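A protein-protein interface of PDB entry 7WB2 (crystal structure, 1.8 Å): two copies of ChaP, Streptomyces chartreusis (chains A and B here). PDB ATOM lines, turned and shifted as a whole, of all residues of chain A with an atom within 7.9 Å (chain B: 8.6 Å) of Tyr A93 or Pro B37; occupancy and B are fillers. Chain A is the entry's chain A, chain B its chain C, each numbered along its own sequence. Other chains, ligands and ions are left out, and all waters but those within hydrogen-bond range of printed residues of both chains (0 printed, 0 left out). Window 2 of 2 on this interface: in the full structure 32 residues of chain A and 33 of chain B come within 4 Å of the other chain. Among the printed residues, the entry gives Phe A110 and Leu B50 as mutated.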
ATOM      1  N   ILE A  60      23.123  17.975   0.138  1.00  0.00           N
ATOM      2  CA  ILE A  60      22.852  16.554  -0.037  1.00  0.00           C
ATOM      3  C   ILE A  60      23.903  15.996  -0.983  1.00  0.00           C
ATOM      4  O   ILE A  60      24.298  16.667  -1.941  1.00  0.00           O
ATOM      5  CB  ILE A  60      21.435  16.303  -0.589  1.00  0.00           C
ATOM      6  N   VAL A  61      24.289  14.875  -0.735  1.00  0.00           N
ATOM      7  CA  VAL A  61      25.385  14.298  -1.494  1.00  0.00           C
ATOM      8  C   VAL A  61      24.922  13.971  -2.912  1.00  0.00           C
ATOM      9  O   VAL A  61      23.748  13.665  -3.134  1.00  0.00           O
ATOM     10  CB  VAL A  61      25.936  13.025  -0.828  1.00  0.00           C
ATOM     11  CG1 VAL A  61      26.410  13.324   0.585  1.00  0.00           C
ATOM     12  CG2 VAL A  61      24.882  11.927  -0.824  1.00  0.00           C
ATOM     13  N   PRO A  62      25.738  14.041  -3.962  1.00  0.00           N
ATOM     14  CA  PRO A  62      27.191  14.187  -3.799  1.00  0.00           C
ATOM     15  C   PRO A  62      27.702  15.626  -3.828  1.00  0.00           C
ATOM     16  O   PRO A  62      28.878  15.837  -4.149  1.00  0.00           O
ATOM     17  CB  PRO A  62      27.734  13.428  -5.002  1.00  0.00           C
ATOM     18  CG  PRO A  62      26.737  13.733  -6.060  1.00  0.00           C
ATOM     19  CD  PRO A  62      25.383  13.782  -5.369  1.00  0.00           C
ATOM     20  N   GLY A  63      26.852  16.596  -3.506  1.00  0.00           N
ATOM     21  CA  GLY A  63      27.330  17.964  -3.411  1.00  0.00           C
ATOM     22  C   GLY A  63      28.372  18.099  -2.316  1.00  0.00           C
ATOM     23  O   GLY A  63      28.283  17.457  -1.270  1.00  0.00           O
ATOM     24  N   HIS A  64      29.374  18.939  -2.571  1.00  0.00           N
ATOM     25  CA  HIS A  64      30.429  19.224  -1.607  1.00  0.00           C
ATOM     26  C   HIS A  64      31.239  20.396  -2.132  1.00  0.00           C
ATOM     27  O   HIS A  64      31.159  20.740  -3.313  1.00  0.00           O
ATOM     28  CB  HIS A  64      31.339  18.009  -1.369  1.00  0.00           C
ATOM     29  CG  HIS A  64      31.983  17.476  -2.613  1.00  0.00           C
ATOM     30  ND1 HIS A  64      31.328  16.642  -3.491  1.00  0.00           N
ATOM     31  CD2 HIS A  64      33.236  17.633  -3.106  1.00  0.00           C
ATOM     32  CE1 HIS A  64      32.139  16.333  -4.489  1.00  0.00           C
ATOM     33  NE2 HIS A  64      33.307  16.913  -4.275  1.00  0.00           N
ATOM     34  N   TRP A  89      34.264   9.918   5.082  1.00  0.00           N
ATOM     35  CA  TRP A  89      34.056   8.924   4.043  1.00  0.00           C
ATOM     36  C   TRP A  89      35.073   9.140   2.939  1.00  0.00           C
ATOM     37  O   TRP A  89      35.566  10.252   2.738  1.00  0.00           O
ATOM     38  CB  TRP A  89      32.623   8.949   3.455  1.00  0.00           C
ATOM     39  CG  TRP A  89      31.533   8.940   4.487  1.00  0.00           C
ATOM     40  CD1 TRP A  89      30.653   7.926   4.725  1.00  0.00           C
ATOM     41  CD2 TRP A  89      31.109  10.033   5.319  1.00  0.00           C
ATOM     42  NE1 TRP A  89      29.776   8.277   5.724  1.00  0.00           N
ATOM     43  CE2 TRP A  89      30.025   9.573   6.091  1.00  0.00           C
ATOM     44  CE3 TRP A  89      31.558  11.344   5.506  1.00  0.00           C
ATOM     45  CZ2 TRP A  89      29.387  10.376   7.036  1.00  0.00           C
ATOM     46  CZ3 TRP A  89      30.932  12.132   6.456  1.00  0.00           C
ATOM     47  CH2 TRP A  89      29.857  11.651   7.201  1.00  0.00           C
ATOM     48  N   ALA A  90      35.377   8.064   2.220  1.00  0.00           N
ATOM     49  CA  ALA A  90      36.309   8.136   1.104  1.00  0.00           C
ATOM     50  C   ALA A  90      35.684   8.684  -0.172  1.00  0.00           C
ATOM     51  O   ALA A  90      36.419   8.971  -1.125  1.00  0.00           O
ATOM     52  CB  ALA A  90      36.910   6.753   0.831  1.00  0.00           C
ATOM     53  N   ASP A  91      34.359   8.832  -0.219  1.00  0.00           N
ATOM     54  CA  ASP A  91      33.638   9.062  -1.464  1.00  0.00           C
ATOM     55  C   ASP A  91      32.632  10.188  -1.295  1.00  0.00           C
ATOM     56  O   ASP A  91      32.107  10.408  -0.205  1.00  0.00           O
ATOM     57  CB  ASP A  91      32.908   7.794  -1.911  1.00  0.00           C
ATOM     58  CG  ASP A  91      31.838   7.379  -0.938  1.00  0.00           C
ATOM     59  OD1 ASP A  91      32.157   7.234   0.258  1.00  0.00           O
ATOM     60  OD2 ASP A  91      30.678   7.203  -1.360  1.00  0.00           O
ATOM     61  N   GLN A  92      32.355  10.891  -2.399  1.00  0.00           N
ATOM     62  CA  GLN A  92      31.438  12.028  -2.361  1.00  0.00           C
ATOM     63  C   GLN A  92      30.010  11.635  -2.018  1.00  0.00           C
ATOM     64  O   GLN A  92      29.224  12.506  -1.633  1.00  0.00           O
ATOM     65  CB  GLN A  92      31.448  12.763  -3.699  1.00  0.00           C
ATOM     66  CG  GLN A  92      30.954  11.911  -4.848  1.00  0.00           C
ATOM     67  CD  GLN A  92      31.017  12.636  -6.175  1.00  0.00           C
ATOM     68  OE1 GLN A  92      31.608  13.716  -6.284  1.00  0.00           O
ATOM     69  NE2 GLN A  92      30.420  12.037  -7.198  1.00  0.00           N
ATOM     70  N   TYR A  93      29.643  10.365  -2.184  1.00  0.00           N
ATOM     71  CA  TYR A  93      28.303   9.902  -1.837  1.00  0.00           C
ATOM     72  C   TYR A  93      28.189   9.388  -0.403  1.00  0.00           C
ATOM     73  O   TYR A  93      27.100   8.959   0.001  1.00  0.00           O
ATOM     74  CB  TYR A  93      27.860   8.811  -2.818  1.00  0.00           C
ATOM     75  CG  TYR A  93      27.433   9.326  -4.173  1.00  0.00           C
ATOM     76  CD1 TYR A  93      26.157   9.833  -4.374  1.00  0.00           C
ATOM     77  CD2 TYR A  93      28.301   9.285  -5.256  1.00  0.00           C
ATOM     78  CE1 TYR A  93      25.758  10.293  -5.609  1.00  0.00           C
ATOM     79  CE2 TYR A  93      27.914   9.747  -6.503  1.00  0.00           C
ATOM     80  CZ  TYR A  93      26.643  10.252  -6.672  1.00  0.00           C
ATOM     81  OH  TYR A  93      26.253  10.707  -7.907  1.00  0.00           O
ATOM     82  N   HIS A  94      29.280   9.414   0.366  1.00  0.00           N
ATOM     83  CA  HIS A  94      29.291   9.007   1.778  1.00  0.00           C
ATOM     84  C   HIS A  94      28.847   7.555   1.943  1.00  0.00           C
ATOM     85  O   HIS A  94      28.141   7.213   2.891  1.00  0.00           O
ATOM     86  CB  HIS A  94      28.425   9.925   2.651  1.00  0.00           C
ATOM     87  CG  HIS A  94      28.877  11.354   2.684  1.00  0.00           C
ATOM     88  ND1 HIS A  94      28.144  12.350   3.297  1.00  0.00           N
ATOM     89  CD2 HIS A  94      29.961  11.963   2.148  1.00  0.00           C
ATOM     90  CE1 HIS A  94      28.771  13.504   3.158  1.00  0.00           C
ATOM     91  NE2 HIS A  94      29.875  13.298   2.464  1.00  0.00           N
ATOM     92  N   ARG A  95      29.261   6.700   1.012  1.00  0.00           N
ATOM     93  CA  ARG A  95      28.959   5.275   1.046  1.00  0.00           C
ATOM     94  C   ARG A  95      30.123   4.443   1.564  1.00  0.00           C
ATOM     95  O   ARG A  95      29.948   3.242   1.793  1.00  0.00           O
ATOM     96  CB  ARG A  95      28.549   4.788  -0.354  1.00  0.00           C
ATOM     97  CG  ARG A  95      27.404   5.602  -0.952  1.00  0.00           C
ATOM     98  CD  ARG A  95      26.251   4.752  -1.463  1.00  0.00           C
ATOM     99  NE  ARG A  95      25.829   5.196  -2.786  1.00  0.00           N
ATOM    100  CZ  ARG A  95      25.120   4.472  -3.644  1.00  0.00           C
ATOM    101  NH1 ARG A  95      24.710   3.250  -3.346  1.00  0.00           N
ATOM    102  NH2 ARG A  95      24.813   4.992  -4.828  1.00  0.00           N
ATOM    103  N   GLU A  96      31.298   5.053   1.755  1.00  0.00           N
ATOM    104  CA  GLU A  96      32.525   4.366   2.163  1.00  0.00           C
ATOM    105  C   GLU A  96      33.028   4.987   3.464  1.00  0.00           C
ATOM    106  O   GLU A  96      34.047   5.692   3.463  1.00  0.00           O
ATOM    107  CB  GLU A  96      33.611   4.512   1.096  1.00  0.00           C
ATOM    108  CG  GLU A  96      33.180   4.331  -0.356  1.00  0.00           C
ATOM    109  CD  GLU A  96      33.574   3.005  -0.950  1.00  0.00           C
ATOM    110  OE1 GLU A  96      34.166   2.183  -0.220  1.00  0.00           O
ATOM    111  OE2 GLU A  96      33.316   2.796  -2.156  1.00  0.00           O
ATOM    112  N   PHE A 110      36.171  12.840   2.543  1.00  0.00           N
ATOM    113  CA  PHE A 110      34.946  13.615   2.607  1.00  0.00           C
ATOM    114  C   PHE A 110      34.411  13.624   4.030  1.00  0.00           C
ATOM    115  O   PHE A 110      34.540  12.639   4.762  1.00  0.00           O
ATOM    116  CB  PHE A 110      33.898  13.055   1.635  1.00  0.00           C
ATOM    117  CG  PHE A 110      34.338  13.082   0.198  1.00  0.00           C
ATOM    118  CD1 PHE A 110      35.224  12.129  -0.291  1.00  0.00           C
ATOM    119  CD2 PHE A 110      33.887  14.068  -0.662  1.00  0.00           C
ATOM    120  CE1 PHE A 110      35.641  12.156  -1.611  1.00  0.00           C
ATOM    121  CE2 PHE A 110      34.288  14.102  -1.983  1.00  0.00           C
ATOM    122  CZ  PHE A 110      35.172  13.145  -2.462  1.00  0.00           C
ATOM    123  N   ASN A 118      28.683  19.738   3.116  1.00  0.00           N
ATOM    124  CA  ASN A 118      29.602  18.671   2.737  1.00  0.00           C
ATOM    125  C   ASN A 118      30.927  19.237   2.256  1.00  0.00           C
ATOM    126  O   ASN A 118      30.942  20.163   1.440  1.00  0.00           O
ATOM    127  CB  ASN A 118      28.993  17.811   1.638  1.00  0.00           C
ATOM    128  CG  ASN A 118      27.767  17.067   2.098  1.00  0.00           C
ATOM    129  OD1 ASN A 118      27.710  16.605   3.232  1.00  0.00           O
ATOM    130  ND2 ASN A 118      26.790  16.922   1.215  1.00  0.00           N
ATOM    131  N   ILE B  10      30.237  22.151  -5.973  1.00  0.00           N
ATOM    132  CA  ILE B  10      29.087  21.620  -6.690  1.00  0.00           C
ATOM    133  C   ILE B  10      27.917  22.577  -6.523  1.00  0.00           C
ATOM    134  O   ILE B  10      27.622  23.033  -5.409  1.00  0.00           O
ATOM    135  CB  ILE B  10      28.726  20.206  -6.203  1.00  0.00           C
ATOM    136  CG1 ILE B  10      29.645  19.162  -6.843  1.00  0.00           C
ATOM    137  CG2 ILE B  10      27.275  19.876  -6.552  1.00  0.00           C
ATOM    138  CD1 ILE B  10      31.101  19.249  -6.469  1.00  0.00           C
ATOM    139  N   VAL B  11      27.266  22.895  -7.637  1.00  0.00           N
ATOM    140  CA  VAL B  11      26.159  23.840  -7.666  1.00  0.00           C
ATOM    141  C   VAL B  11      24.921  23.089  -8.124  1.00  0.00           C
ATOM    142  O   VAL B  11      24.912  22.504  -9.216  1.00  0.00           O
ATOM    143  CB  VAL B  11      26.459  25.032  -8.583  1.00  0.00           C
ATOM    144  CG1 VAL B  11      25.201  25.838  -8.819  1.00  0.00           C
ATOM    145  CG2 VAL B  11      27.530  25.898  -7.958  1.00  0.00           C
ATOM    146  N   VAL B  13      21.290  22.766  -9.583  1.00  0.00           N
ATOM    147  CA  VAL B  13      20.394  23.494 -10.475  1.00  0.00           C
ATOM    148  C   VAL B  13      19.418  22.511 -11.103  1.00  0.00           C
ATOM    149  O   VAL B  13      19.691  21.315 -11.213  1.00  0.00           O
ATOM    150  CB  VAL B  13      21.143  24.265 -11.583  1.00  0.00           C
ATOM    151  CG1 VAL B  13      22.132  25.257 -10.974  1.00  0.00           C
ATOM    152  CG2 VAL B  13      21.856  23.291 -12.514  1.00  0.00           C
ATOM    153  N   LYS B  16      21.352  20.770 -15.306  1.00  0.00           N
ATOM    154  CA  LYS B  16      22.793  21.011 -15.278  1.00  0.00           C
ATOM    155  C   LYS B  16      23.334  21.342 -16.659  1.00  0.00           C
ATOM    156  O   LYS B  16      24.239  22.173 -16.788  1.00  0.00           O
ATOM    157  CB  LYS B  16      23.531  19.805 -14.689  1.00  0.00           C
ATOM    158  CG  LYS B  16      23.626  18.586 -15.599  1.00  0.00           C
ATOM    159  CD  LYS B  16      24.183  17.388 -14.846  1.00  0.00           C
ATOM    160  CE  LYS B  16      24.812  16.368 -15.786  1.00  0.00           C
ATOM    161  NZ  LYS B  16      24.124  16.296 -17.107  1.00  0.00           N
ATOM    162  N   ASP B  17      22.773  20.728 -17.706  1.00  0.00           N
ATOM    163  CA  ASP B  17      23.259  20.991 -19.055  1.00  0.00           C
ATOM    164  C   ASP B  17      22.874  22.390 -19.512  1.00  0.00           C
ATOM    165  O   ASP B  17      23.686  23.084 -20.128  1.00  0.00           O
ATOM    166  CB  ASP B  17      22.723  19.943 -20.033  1.00  0.00           C
ATOM    167  CG  ASP B  17      23.473  18.625 -19.958  1.00  0.00           C
ATOM    168  OD1 ASP B  17      24.011  18.285 -18.880  1.00  0.00           O
ATOM    169  OD2 ASP B  17      23.525  17.921 -20.992  1.00  0.00           O
ATOM    170  N   LYS B  33      32.646  20.278 -20.024  1.00  0.00           N
ATOM    171  CA  LYS B  33      32.868  18.845 -20.028  1.00  0.00           C
ATOM    172  C   LYS B  33      31.918  18.215 -19.024  1.00  0.00           C
ATOM    173  O   LYS B  33      31.695  18.754 -17.936  1.00  0.00           O
ATOM    174  CB  LYS B  33      34.318  18.511 -19.675  1.00  0.00           C
ATOM    175  N   GLU B  34      31.329  17.089 -19.414  1.00  0.00           N
ATOM    176  CA  GLU B  34      30.414  16.336 -18.571  1.00  0.00           C
ATOM    177  C   GLU B  34      31.130  15.113 -18.003  1.00  0.00           C
ATOM    178  O   GLU B  34      31.765  14.365 -18.751  1.00  0.00           O
ATOM    179  CB  GLU B  34      29.176  15.930 -19.370  1.00  0.00           C
ATOM    180  CG  GLU B  34      27.880  16.133 -18.619  1.00  0.00           C
ATOM    181  CD  GLU B  34      26.686  16.258 -19.550  1.00  0.00           C
ATOM    182  OE1 GLU B  34      26.761  17.068 -20.498  1.00  0.00           O
ATOM    183  OE2 GLU B  34      25.677  15.555 -19.333  1.00  0.00           O
ATOM    184  N   MET B  35      31.045  14.928 -16.684  1.00  0.00           N
ATOM    185  CA  MET B  35      31.709  13.816 -16.004  1.00  0.00           C
ATOM    186  C   MET B  35      30.824  13.320 -14.873  1.00  0.00           C
ATOM    187  O   MET B  35      30.592  14.048 -13.903  1.00  0.00           O
ATOM    188  CB  MET B  35      33.082  14.229 -15.456  1.00  0.00           C
ATOM    189  N   GLY B  36      30.368  12.071 -14.972  1.00  0.00           N
ATOM    190  CA  GLY B  36      29.423  11.529 -14.023  1.00  0.00           C
ATOM    191  C   GLY B  36      28.159  12.360 -13.931  1.00  0.00           C
ATOM    192  O   GLY B  36      27.510  12.661 -14.941  1.00  0.00           O
ATOM    193  N   PRO B  37      27.769  12.739 -12.712  1.00  0.00           N
ATOM    194  CA  PRO B  37      26.580  13.575 -12.540  1.00  0.00           C
ATOM    195  C   PRO B  37      26.825  15.066 -12.706  1.00  0.00           C
ATOM    196  O   PRO B  37      25.928  15.853 -12.393  1.00  0.00           O
ATOM    197  CB  PRO B  37      26.164  13.262 -11.095  1.00  0.00           C
ATOM    198  CG  PRO B  37      27.454  13.013 -10.393  1.00  0.00           C
ATOM    199  CD  PRO B  37      28.418  12.434 -11.425  1.00  0.00           C
ATOM    200  N   PHE B  38      28.005  15.479 -13.162  1.00  0.00           N
ATOM    201  CA  PHE B  38      28.381  16.884 -13.170  1.00  0.00           C
ATOM    202  C   PHE B  38      28.577  17.411 -14.584  1.00  0.00           C
ATOM    203  O   PHE B  38      29.116  16.721 -15.456  1.00  0.00           O
ATOM    204  CB  PHE B  38      29.672  17.121 -12.376  1.00  0.00           C
ATOM    205  CG  PHE B  38      29.620  16.611 -10.968  1.00  0.00           C
ATOM    206  CD1 PHE B  38      28.698  17.119 -10.078  1.00  0.00           C
ATOM    207  CD2 PHE B  38      30.498  15.632 -10.531  1.00  0.00           C
ATOM    208  CE1 PHE B  38      28.638  16.655  -8.784  1.00  0.00           C
ATOM    209  CE2 PHE B  38      30.446  15.167  -9.230  1.00  0.00           C
ATOM    210  CZ  PHE B  38      29.511  15.682  -8.357  1.00  0.00           C
ATOM    211  N   ALA B  39      28.179  18.662 -14.777  1.00  0.00           N
ATOM    212  CA  ALA B  39      28.584  19.458 -15.925  1.00  0.00           C
ATOM    213  C   ALA B  39      29.630  20.441 -15.420  1.00  0.00           C
ATOM    214  O   ALA B  39      29.350  21.241 -14.520  1.00  0.00           O
ATOM    215  CB  ALA B  39      27.397  20.187 -16.553  1.00  0.00           C
ATOM    216  N   VAL B  40      30.826  20.383 -15.985  1.00  0.00           N
ATOM    217  CA  VAL B  40      31.957  21.049 -15.360  1.00  0.00           C
ATOM    218  C   VAL B  40      32.252  22.334 -16.110  1.00  0.00           C
ATOM    219  O   VAL B  40      32.400  22.334 -17.341  1.00  0.00           O
ATOM    220  CB  VAL B  40      33.199  20.143 -15.333  1.00  0.00           C
ATOM    221  CG1 VAL B  40      34.342  20.864 -14.629  1.00  0.00           C
ATOM    222  CG2 VAL B  40      32.868  18.823 -14.654  1.00  0.00           C
ATOM    223  N   LEU B  50      30.872  22.604 -10.611  1.00  0.00           N
ATOM    224  CA  LEU B  50      30.329  21.327 -11.052  1.00  0.00           C
ATOM    225  C   LEU B  50      28.812  21.404 -10.897  1.00  0.00           C
ATOM    226  O   LEU B  50      28.279  21.242  -9.795  1.00  0.00           O
ATOM    227  CB  LEU B  50      30.922  20.189 -10.228  1.00  0.00           C
ATOM    228  CG  LEU B  50      32.179  19.489 -10.732  1.00  0.00           C
ATOM    229  CD1 LEU B  50      33.177  20.478 -11.343  1.00  0.00           C
ATOM    230  CD2 LEU B  50      32.814  18.714  -9.571  1.00  0.00           C
ATOM    231  N   PHE B  51      28.119  21.644 -12.007  1.00  0.00           N
ATOM    232  CA  PHE B  51      26.668  21.776 -11.986  1.00  0.00           C
ATOM    233  C   PHE B  51      26.045  20.390 -11.879  1.00  0.00           C
ATOM    234  O   PHE B  51      26.507  19.447 -12.524  1.00  0.00           O
ATOM    235  CB  PHE B  51      26.185  22.450 -13.267  1.00  0.00           C
ATOM    236  CG  PHE B  51      26.387  23.938 -13.289  1.00  0.00           C
ATOM    237  CD1 PHE B  51      25.441  24.799 -12.765  1.00  0.00           C
ATOM    238  CD2 PHE B  51      27.511  24.476 -13.901  1.00  0.00           C
ATOM    239  CE1 PHE B  51      25.634  26.167 -12.808  1.00  0.00           C
ATOM    240  CE2 PHE B  51      27.707  25.847 -13.953  1.00  0.00           C
ATOM    241  CZ  PHE B  51      26.769  26.692 -13.401  1.00  0.00           C
ATOM    242  N   MET B  52      24.996  20.262 -11.067  1.00  0.00           N
ATOM    243  CA  MET B  52      24.343  18.971 -10.905  1.00  0.00           C
ATOM    244  C   MET B  52      22.833  19.157 -10.865  1.00  0.00           C
ATOM    245  O   MET B  52      22.339  20.104 -10.247  1.00  0.00           O
ATOM    246  CB  MET B  52      24.817  18.274  -9.630  1.00  0.00           C
ATOM    247  CG  MET B  52      24.188  16.913  -9.392  1.00  0.00           C
ATOM    248  SD  MET B  52      24.960  16.060  -8.016  1.00  0.00           S
ATOM    249  CE  MET B  52      24.638  17.208  -6.681  1.00  0.00           C
ATOM    250  N   ASP B  53      22.106  18.242 -11.512  1.00  0.00           N
ATOM    251  CA  ASP B  53      20.645  18.305 -11.527  1.00  0.00           C
ATOM    252  C   ASP B  53      20.074  18.168 -10.121  1.00  0.00           C
ATOM    253  O   ASP B  53      20.502  17.311  -9.341  1.00  0.00           O
ATOM    254  CB  ASP B  53      20.067  17.199 -12.417  1.00  0.00           C
ATOM    255  CG  ASP B  53      20.466  17.346 -13.869  1.00  0.00           C
ATOM    256  OD1 ASP B  53      20.635  18.492 -14.319  1.00  0.00           O
ATOM    257  OD2 ASP B  53      20.629  16.315 -14.559  1.00  0.00           O
ATOM    258  N   PHE B  54      19.098  19.018  -9.801  1.00  0.00           N
ATOM    259  CA  PHE B  54      18.367  18.931  -8.540  1.00  0.00           C
ATOM    260  C   PHE B  54      16.968  19.489  -8.744  1.00  0.00           C
ATOM    261  O   PHE B  54      16.804  20.559  -9.337  1.00  0.00           O
ATOM    262  CB  PHE B  54      19.076  19.693  -7.415  1.00  0.00           C
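The backbone carbonyl oxygen (O) of His A64 is in hydrogen-bond range of the backbone NH (N) of Ile B10, 3.1 Å away.
A ring nitrogen (ND1) of His A64 lies within hydrogen-bond range of the backbone carbonyl oxygen (O) of Pro A62. The backbone carbonyl oxygen (O) of Gly A63 is in hydrogen-bond range of the side-chain amide nitrogen (ND2) of Asn A118. The side-chain carboxylate (OD2) of Asp A91 lies close to the backbone NH (N) of Tyr A93, 3.4 Å away. O of Val B11 sits at hydrogen-bond distance from N of Met B52, 2.9 Å away. N of Val B13 is in hydrogen-bond range of O of Met B52 (2.9 Å).
Among the printed residues, merely in contact across the chains: Pro A62 with Met B52, Gly A63 with Ile B10, Gly A63 with Met B52, Gln A92 with Phe B38 and Tyr A93 with Pro B37.
Of the printed residues of chain B, Pro A62 touches Met B52 (3.5 Å). Of the printed residues of chain B, Gly A63 touches Ile B10 and Met B52. Printed residues of chain A within 4 Å of Ile B10: Gly A63 and His A64. Printed residues of chain A within 4 Å of Pro B37: Tyr A93 (3.6 Å). Printed residues of chain A within 4 Å of Met B52: Pro A62 (3.5 Å) and Gly A63 (3.9 Å).
Printed residues of chain A that touch a printed residue of chain B: Pro A62, Gly A63, His A64, Gln A92 and Tyr A93. Hydrophobic or aromatic side chains of chain A that line the printed part of chain B: Pro A62, His A64 and Tyr A93. Printed residues of chain B that touch a printed residue of chain A: Ile B10, Pro B37, Phe B38 and Met B52. Among the printed residues, no Asp or Glu carboxylate lies within 4 Å of a Lys or Arg side-chain nitrogen of the other chain.
No position is printed for both chains.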
